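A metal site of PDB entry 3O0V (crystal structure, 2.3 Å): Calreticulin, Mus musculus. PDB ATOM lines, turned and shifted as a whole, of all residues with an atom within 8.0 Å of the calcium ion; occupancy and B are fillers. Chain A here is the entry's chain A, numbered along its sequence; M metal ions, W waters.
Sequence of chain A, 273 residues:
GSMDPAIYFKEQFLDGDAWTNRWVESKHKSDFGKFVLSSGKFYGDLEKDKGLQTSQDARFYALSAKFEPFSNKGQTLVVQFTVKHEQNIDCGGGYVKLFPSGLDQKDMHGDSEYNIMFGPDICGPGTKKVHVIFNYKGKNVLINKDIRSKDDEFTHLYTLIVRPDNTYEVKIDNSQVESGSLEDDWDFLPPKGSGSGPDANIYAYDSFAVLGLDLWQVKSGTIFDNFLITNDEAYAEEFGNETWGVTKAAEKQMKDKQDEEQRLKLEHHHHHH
Of the 24 residues printed, 4 come within 4 Å of the calcium ion.
The side-chain amide nitrogen of Gln 12 sits close to the side-chain amide nitrogen of Asn 226, at 3.3 Å. The side-chain carboxylate (OD1) of Asp 45 lies within hydrogen-bond range of the backbone NH (N) of Lys 48, at 2.9 Å. The side-chain amino group (NZ) of Lys 50 is in hydrogen-bond range of the backbone carbonyl oxygen (O) of Leu 46 (2.9 Å). OE2 of Glu 47 is in salt-bridge range of NZ of Lys 50 (3.7 Å). O of Asp 225 sits at hydrogen-bond distance from N of Thr 82 (2.9 Å).
The calcium ion is bound by the backbone carbonyl oxygen (O) of Lys 48 (2.4 Å), the backbone carbonyl oxygen (O) of Gln 12 (2.4 Å), water W1 (2.4 Å), the side-chain carboxylate (OD1) of Asp 225 (2.5 Å), water W2 (2.5 Å), the backbone carbonyl oxygen (O) of Lys 50 (2.6 Å) and the side-chain carboxylate (OD2) of Asp 225 (2.6 Å). The calcium ion has seven donor atoms within binding distance.
Water W2 bridges the backbone carbonyl oxygen of Glu 47 (2.6 Å) and the backbone carbonyl oxygen of Phe 13 (2.8 Å).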
ATOM      1  N   GLU A  11      21.745   4.916  27.638  1.00  0.00           N
ATOM      2  CA  GLU A  11      20.534   4.337  28.209  1.00  0.00           C
ATOM      3  C   GLU A  11      19.691   3.699  27.124  1.00  0.00           C
ATOM      4  O   GLU A  11      19.277   4.357  26.169  1.00  0.00           O
ATOM      5  CB  GLU A  11      19.734   5.394  28.973  1.00  0.00           C
ATOM      6  CG  GLU A  11      18.439   4.879  29.580  1.00  0.00           C
ATOM      7  CD  GLU A  11      18.663   3.996  30.805  1.00  0.00           C
ATOM      8  OE1 GLU A  11      18.892   4.553  31.906  1.00  0.00           O
ATOM      9  OE2 GLU A  11      18.585   2.756  30.678  1.00  0.00           O
ATOM     10  N   GLN A  12      19.439   2.397  27.278  1.00  0.00           N
ATOM     11  CA  GLN A  12      18.633   1.646  26.319  1.00  0.00           C
ATOM     12  C   GLN A  12      17.451   0.941  26.982  1.00  0.00           C
ATOM     13  O   GLN A  12      16.662   0.278  26.299  1.00  0.00           O
ATOM     14  CB  GLN A  12      19.498   0.632  25.561  1.00  0.00           C
ATOM     15  CG  GLN A  12      20.693   1.213  24.845  1.00  0.00           C
ATOM     16  CD  GLN A  12      21.503   0.148  24.138  1.00  0.00           C
ATOM     17  OE1 GLN A  12      22.535  -0.313  24.638  1.00  0.00           O
ATOM     18  NE2 GLN A  12      21.037  -0.275  22.973  1.00  0.00           N
ATOM     19  N   PHE A  13      17.327   1.098  28.303  1.00  0.00           N
ATOM     20  CA  PHE A  13      16.223   0.506  29.062  1.00  0.00           C
ATOM     21  C   PHE A  13      16.080  -0.993  28.809  1.00  0.00           C
ATOM     22  O   PHE A  13      15.012  -1.469  28.420  1.00  0.00           O
ATOM     23  CB  PHE A  13      14.892   1.231  28.764  1.00  0.00           C
ATOM     24  CG  PHE A  13      14.983   2.731  28.802  1.00  0.00           C
ATOM     25  CD1 PHE A  13      14.933   3.417  30.012  1.00  0.00           C
ATOM     26  CD2 PHE A  13      15.094   3.466  27.615  1.00  0.00           C
ATOM     27  CE1 PHE A  13      15.009   4.808  30.045  1.00  0.00           C
ATOM     28  CE2 PHE A  13      15.171   4.849  27.632  1.00  0.00           C
ATOM     29  CZ  PHE A  13      15.133   5.528  28.853  1.00  0.00           C
ATOM     30  N   LEU A  14      17.169  -1.737  29.029  1.00  0.00           N
ATOM     31  CA  LEU A  14      17.202  -3.167  28.711  1.00  0.00           C
ATOM     32  C   LEU A  14      16.935  -4.091  29.915  1.00  0.00           C
ATOM     33  O   LEU A  14      16.797  -5.306  29.749  1.00  0.00           O
ATOM     34  CB  LEU A  14      18.543  -3.541  28.065  1.00  0.00           C
ATOM     35  CG  LEU A  14      18.889  -2.940  26.694  1.00  0.00           C
ATOM     36  CD1 LEU A  14      20.397  -2.987  26.451  1.00  0.00           C
ATOM     37  CD2 LEU A  14      18.134  -3.626  25.573  1.00  0.00           C
ATOM     38  N   ASP A  15      16.852  -3.500  31.110  1.00  0.00           N
ATOM     39  CA  ASP A  15      16.802  -4.281  32.360  1.00  0.00           C
ATOM     40  C   ASP A  15      15.540  -4.072  33.209  1.00  0.00           C
ATOM     41  O   ASP A  15      15.616  -3.970  34.439  1.00  0.00           O
ATOM     42  CB  ASP A  15      18.064  -3.991  33.197  1.00  0.00           C
ATOM     43  CG  ASP A  15      18.198  -2.525  33.582  1.00  0.00           C
ATOM     44  OD1 ASP A  15      17.538  -1.658  32.953  1.00  0.00           O
ATOM     45  OD2 ASP A  15      18.977  -2.219  34.513  1.00  0.00           O
ATOM     46  N   LEU A  37       7.519   2.688  31.073  1.00  0.00           N
ATOM     47  CA  LEU A  37       8.358   1.808  30.252  1.00  0.00           C
ATOM     48  C   LEU A  37       7.477   1.050  29.267  1.00  0.00           C
ATOM     49  O   LEU A  37       6.624   0.240  29.660  1.00  0.00           O
ATOM     50  CB  LEU A  37       9.164   0.839  31.125  1.00  0.00           C
ATOM     51  CG  LEU A  37      10.168  -0.072  30.405  1.00  0.00           C
ATOM     52  CD1 LEU A  37      11.374   0.704  29.859  1.00  0.00           C
ATOM     53  CD2 LEU A  37      10.636  -1.185  31.327  1.00  0.00           C
ATOM     54  N   SER A  38       7.661   1.328  27.978  1.00  0.00           N
ATOM     55  CA  SER A  38       6.816   0.741  26.945  1.00  0.00           C
ATOM     56  C   SER A  38       7.526   0.529  25.608  1.00  0.00           C
ATOM     57  O   SER A  38       8.451   1.255  25.259  1.00  0.00           O
ATOM     58  CB  SER A  38       5.550   1.594  26.746  1.00  0.00           C
ATOM     59  OG  SER A  38       4.771   1.126  25.656  1.00  0.00           O
ATOM     60  N   SER A  39       7.047  -0.479  24.894  1.00  0.00           N
ATOM     61  CA  SER A  39       7.560  -0.882  23.595  1.00  0.00           C
ATOM     62  C   SER A  39       6.549  -0.481  22.505  1.00  0.00           C
ATOM     63  O   SER A  39       6.855  -0.521  21.311  1.00  0.00           O
ATOM     64  CB  SER A  39       7.771  -2.395  23.601  1.00  0.00           C
ATOM     65  OG  SER A  39       8.079  -2.921  22.317  1.00  0.00           O
ATOM     66  N   ASP A  45      11.453  -4.896  17.913  1.00  0.00           N
ATOM     67  CA  ASP A  45      11.612  -5.994  18.861  1.00  0.00           C
ATOM     68  C   ASP A  45      10.943  -5.598  20.170  1.00  0.00           C
ATOM     69  O   ASP A  45      11.154  -4.482  20.667  1.00  0.00           O
ATOM     70  CB  ASP A  45      13.098  -6.302  19.069  1.00  0.00           C
ATOM     71  CG  ASP A  45      13.333  -7.459  20.029  1.00  0.00           C
ATOM     72  OD1 ASP A  45      13.518  -7.195  21.238  1.00  0.00           O
ATOM     73  OD2 ASP A  45      13.319  -8.616  19.577  1.00  0.00           O
ATOM     74  N   LEU A  46      10.132  -6.501  20.724  1.00  0.00           N
ATOM     75  CA  LEU A  46       9.341  -6.228  21.930  1.00  0.00           C
ATOM     76  C   LEU A  46      10.188  -5.723  23.108  1.00  0.00           C
ATOM     77  O   LEU A  46       9.787  -4.790  23.789  1.00  0.00           O
ATOM     78  CB  LEU A  46       8.523  -7.455  22.340  1.00  0.00           C
ATOM     79  CG  LEU A  46       7.657  -7.405  23.603  1.00  0.00           C
ATOM     80  CD1 LEU A  46       6.453  -6.502  23.426  1.00  0.00           C
ATOM     81  CD2 LEU A  46       7.200  -8.801  24.011  1.00  0.00           C
ATOM     82  N   GLU A  47      11.339  -6.342  23.332  1.00  0.00           N
ATOM     83  CA  GLU A  47      12.186  -5.981  24.477  1.00  0.00           C
ATOM     84  C   GLU A  47      13.193  -4.871  24.162  1.00  0.00           C
ATOM     85  O   GLU A  47      13.399  -3.977  24.983  1.00  0.00           O
ATOM     86  CB  GLU A  47      12.900  -7.214  25.062  1.00  0.00           C
ATOM     87  CG  GLU A  47      11.972  -8.199  25.773  1.00  0.00           C
ATOM     88  CD  GLU A  47      11.253  -7.598  26.980  1.00  0.00           C
ATOM     89  OE1 GLU A  47      11.829  -6.732  27.679  1.00  0.00           O
ATOM     90  OE2 GLU A  47      10.100  -8.010  27.248  1.00  0.00           O
ATOM     91  N   LYS A  48      13.806  -4.940  22.982  1.00  0.00           N
ATOM     92  CA  LYS A  48      14.830  -3.959  22.590  1.00  0.00           C
ATOM     93  C   LYS A  48      14.272  -2.558  22.448  1.00  0.00           C
ATOM     94  O   LYS A  48      14.947  -1.566  22.785  1.00  0.00           O
ATOM     95  CB  LYS A  48      15.505  -4.375  21.272  1.00  0.00           C
ATOM     96  CG  LYS A  48      16.474  -5.548  21.398  1.00  0.00           C
ATOM     97  CD  LYS A  48      17.013  -5.963  20.030  1.00  0.00           C
ATOM     98  CE  LYS A  48      17.563  -7.379  20.055  1.00  0.00           C
ATOM     99  NZ  LYS A  48      18.182  -7.767  18.749  1.00  0.00           N
ATOM    100  N   ASP A  49      13.035  -2.455  21.964  1.00  0.00           N
ATOM    101  CA  ASP A  49      12.417  -1.164  21.674  1.00  0.00           C
ATOM    102  C   ASP A  49      11.561  -0.598  22.810  1.00  0.00           C
ATOM    103  O   ASP A  49      10.801   0.361  22.603  1.00  0.00           O
ATOM    104  CB  ASP A  49      11.642  -1.229  20.358  1.00  0.00           C
ATOM    105  CG  ASP A  49      12.551  -1.352  19.151  1.00  0.00           C
ATOM    106  OD1 ASP A  49      13.601  -0.676  19.127  1.00  0.00           O
ATOM    107  OD2 ASP A  49      12.234  -2.141  18.238  1.00  0.00           O
ATOM    108  N   LYS A  50      11.683  -1.190  24.002  1.00  0.00           N
ATOM    109  CA  LYS A  50      11.152  -0.585  25.218  1.00  0.00           C
ATOM    110  C   LYS A  50      11.872   0.733  25.477  1.00  0.00           C
ATOM    111  O   LYS A  50      13.109   0.789  25.460  1.00  0.00           O
ATOM    112  CB  LYS A  50      11.336  -1.503  26.436  1.00  0.00           C
ATOM    113  CG  LYS A  50      10.574  -2.833  26.417  1.00  0.00           C
ATOM    114  CD  LYS A  50       9.177  -2.701  27.008  1.00  0.00           C
ATOM    115  CE  LYS A  50       8.609  -4.060  27.417  1.00  0.00           C
ATOM    116  NZ  LYS A  50       8.338  -4.969  26.253  1.00  0.00           N
ATOM    117  N   GLY A  51      11.100   1.793  25.698  1.00  0.00           N
ATOM    118  CA  GLY A  51      11.645   3.085  26.116  1.00  0.00           C
ATOM    119  C   GLY A  51      10.691   3.818  27.035  1.00  0.00           C
ATOM    120  O   GLY A  51       9.685   3.256  27.474  1.00  0.00           O
ATOM    121  N   LEU A  52      10.995   5.080  27.321  1.00  0.00           N
ATOM    122  CA  LEU A  52      10.111   5.925  28.121  1.00  0.00           C
ATOM    123  C   LEU A  52       9.001   6.514  27.270  1.00  0.00           C
ATOM    124  O   LEU A  52       9.256   7.257  26.316  1.00  0.00           O
ATOM    125  CB  LEU A  52      10.908   7.036  28.817  1.00  0.00           C
ATOM    126  CG  LEU A  52      11.947   6.606  29.854  1.00  0.00           C
ATOM    127  CD1 LEU A  52      12.809   7.798  30.284  1.00  0.00           C
ATOM    128  CD2 LEU A  52      11.317   5.920  31.050  1.00  0.00           C
ATOM    129  N   THR A  82      16.663   8.327  20.066  1.00  0.00           N
ATOM    130  CA  THR A  82      15.573   8.074  19.122  1.00  0.00           C
ATOM    131  C   THR A  82      14.266   8.632  19.668  1.00  0.00           C
ATOM    132  O   THR A  82      14.032   8.650  20.881  1.00  0.00           O
ATOM    133  CB  THR A  82      15.420   6.567  18.768  1.00  0.00           C
ATOM    134  OG1 THR A  82      15.132   5.809  19.951  1.00  0.00           O
ATOM    135  CG2 THR A  82      16.665   6.026  18.108  1.00  0.00           C
ATOM    136  N   ILE A 223       7.581   7.787  22.531  1.00  0.00           N
ATOM    137  CA  ILE A 223       8.585   6.919  23.151  1.00  0.00           C
ATOM    138  C   ILE A 223      10.014   7.430  22.887  1.00  0.00           C
ATOM    139  O   ILE A 223      10.361   7.770  21.750  1.00  0.00           O
ATOM    140  CB  ILE A 223       8.461   5.427  22.696  1.00  0.00           C
ATOM    141  CG1 ILE A 223       7.038   4.905  22.921  1.00  0.00           C
ATOM    142  CG2 ILE A 223       9.465   4.547  23.452  1.00  0.00           C
ATOM    143  CD1 ILE A 223       6.819   3.443  22.491  1.00  0.00           C
ATOM    144  N   PHE A 224      10.814   7.468  23.947  1.00  0.00           N
ATOM    145  CA  PHE A 224      12.218   7.884  23.883  1.00  0.00           C
ATOM    146  C   PHE A 224      13.107   6.691  24.210  1.00  0.00           C
ATOM    147  O   PHE A 224      12.840   5.974  25.174  1.00  0.00           O
ATOM    148  CB  PHE A 224      12.496   9.001  24.881  1.00  0.00           C
ATOM    149  CG  PHE A 224      11.755  10.273  24.604  1.00  0.00           C
ATOM    150  CD1 PHE A 224      10.509  10.519  25.184  1.00  0.00           C
ATOM    151  CD2 PHE A 224      12.299  11.249  23.767  1.00  0.00           C
ATOM    152  CE1 PHE A 224       9.815  11.691  24.924  1.00  0.00           C
ATOM    153  CE2 PHE A 224      11.614  12.430  23.503  1.00  0.00           C
ATOM    154  CZ  PHE A 224      10.375  12.656  24.074  1.00  0.00           C
ATOM    155  N   ASP A 225      14.160   6.495  23.426  1.00  0.00           N
ATOM    156  CA  ASP A 225      15.024   5.318  23.567  1.00  0.00           C
ATOM    157  C   ASP A 225      16.439   5.613  23.097  1.00  0.00           C
ATOM    158  O   ASP A 225      16.690   6.626  22.444  1.00  0.00           O
ATOM    159  CB  ASP A 225      14.417   4.165  22.760  1.00  0.00           C
ATOM    160  CG  ASP A 225      14.903   2.788  23.212  1.00  0.00           C
ATOM    161  OD1 ASP A 225      15.645   2.665  24.215  1.00  0.00           O
ATOM    162  OD2 ASP A 225      14.504   1.807  22.560  1.00  0.00           O
ATOM    163  N   ASN A 226      17.375   4.727  23.465  1.00  0.00           N
ATOM    164  CA  ASN A 226      18.745   4.694  22.932  1.00  0.00           C
ATOM    165  C   ASN A 226      19.499   6.020  23.029  1.00  0.00           C
ATOM    166  O   ASN A 226      20.018   6.532  22.035  1.00  0.00           O
ATOM    167  CB  ASN A 226      18.754   4.180  21.477  1.00  0.00           C
ATOM    168  CG  ASN A 226      18.166   2.792  21.346  1.00  0.00           C
ATOM    169  OD1 ASN A 226      17.276   2.563  20.519  1.00  0.00           O
ATOM    170  ND2 ASN A 226      18.657   1.859  22.149  1.00  0.00           N
ATOM    171  N   PHE A 227      19.531   6.575  24.237  1.00  0.00           N
ATOM    172  CA  PHE A 227      20.272   7.792  24.529  1.00  0.00           C
ATOM    173  C   PHE A 227      21.770   7.524  24.491  1.00  0.00           C
ATOM    174  O   PHE A 227      22.250   6.529  25.046  1.00  0.00           O
ATOM    175  CB  PHE A 227      19.887   8.329  25.914  1.00  0.00           C
ATOM    176  CG  PHE A 227      18.450   8.799  26.021  1.00  0.00           C
ATOM    177  CD1 PHE A 227      18.117  10.112  25.742  1.00  0.00           C
ATOM    178  CD2 PHE A 227      17.443   7.919  26.403  1.00  0.00           C
ATOM    179  CE1 PHE A 227      16.793  10.550  25.840  1.00  0.00           C
ATOM    180  CE2 PHE A 227      16.115   8.347  26.518  1.00  0.00           C
ATOM    181  CZ  PHE A 227      15.800   9.669  26.225  1.00  0.00           C
ATOM    182  N   THR A 243      21.168   0.310  16.557  1.00  0.00           N
ATOM    183  CA  THR A 243      20.072   0.646  17.441  1.00  0.00           C
ATOM    184  C   THR A 243      18.834   1.065  16.625  1.00  0.00           C
ATOM    185  O   THR A 243      17.921   0.253  16.447  1.00  0.00           O
ATOM    186  CB  THR A 243      20.565   1.690  18.508  1.00  0.00           C
ATOM    187  OG1 THR A 243      20.198   1.265  19.828  1.00  0.00           O
ATOM    188  CG2 THR A 243      20.108   3.109  18.240  1.00  0.00           C
ATOM    189  N   THR A 247      15.958  -1.308  14.384  1.00  0.00           N
ATOM    190  CA  THR A 247      14.552  -1.036  14.696  1.00  0.00           C
ATOM    191  C   THR A 247      13.714  -0.827  13.431  1.00  0.00           C
ATOM    192  O   THR A 247      12.609  -1.377  13.320  1.00  0.00           O
ATOM    193  CB  THR A 247      14.404   0.211  15.622  1.00  0.00           C
ATOM    194  OG1 THR A 247      15.091  -0.027  16.851  1.00  0.00           O
ATOM    195  CG2 THR A 247      12.941   0.508  15.908  1.00  0.00           C
HETATM  196 CA    CA M   1      15.342   0.147  24.345  1.00  0.00          CA
HETATM  197  O   HOH W   1      17.211  -0.242  22.876  1.00  0.00           O
HETATM  198  O   HOH W   2      14.943  -1.977  25.687  1.00  0.00           O
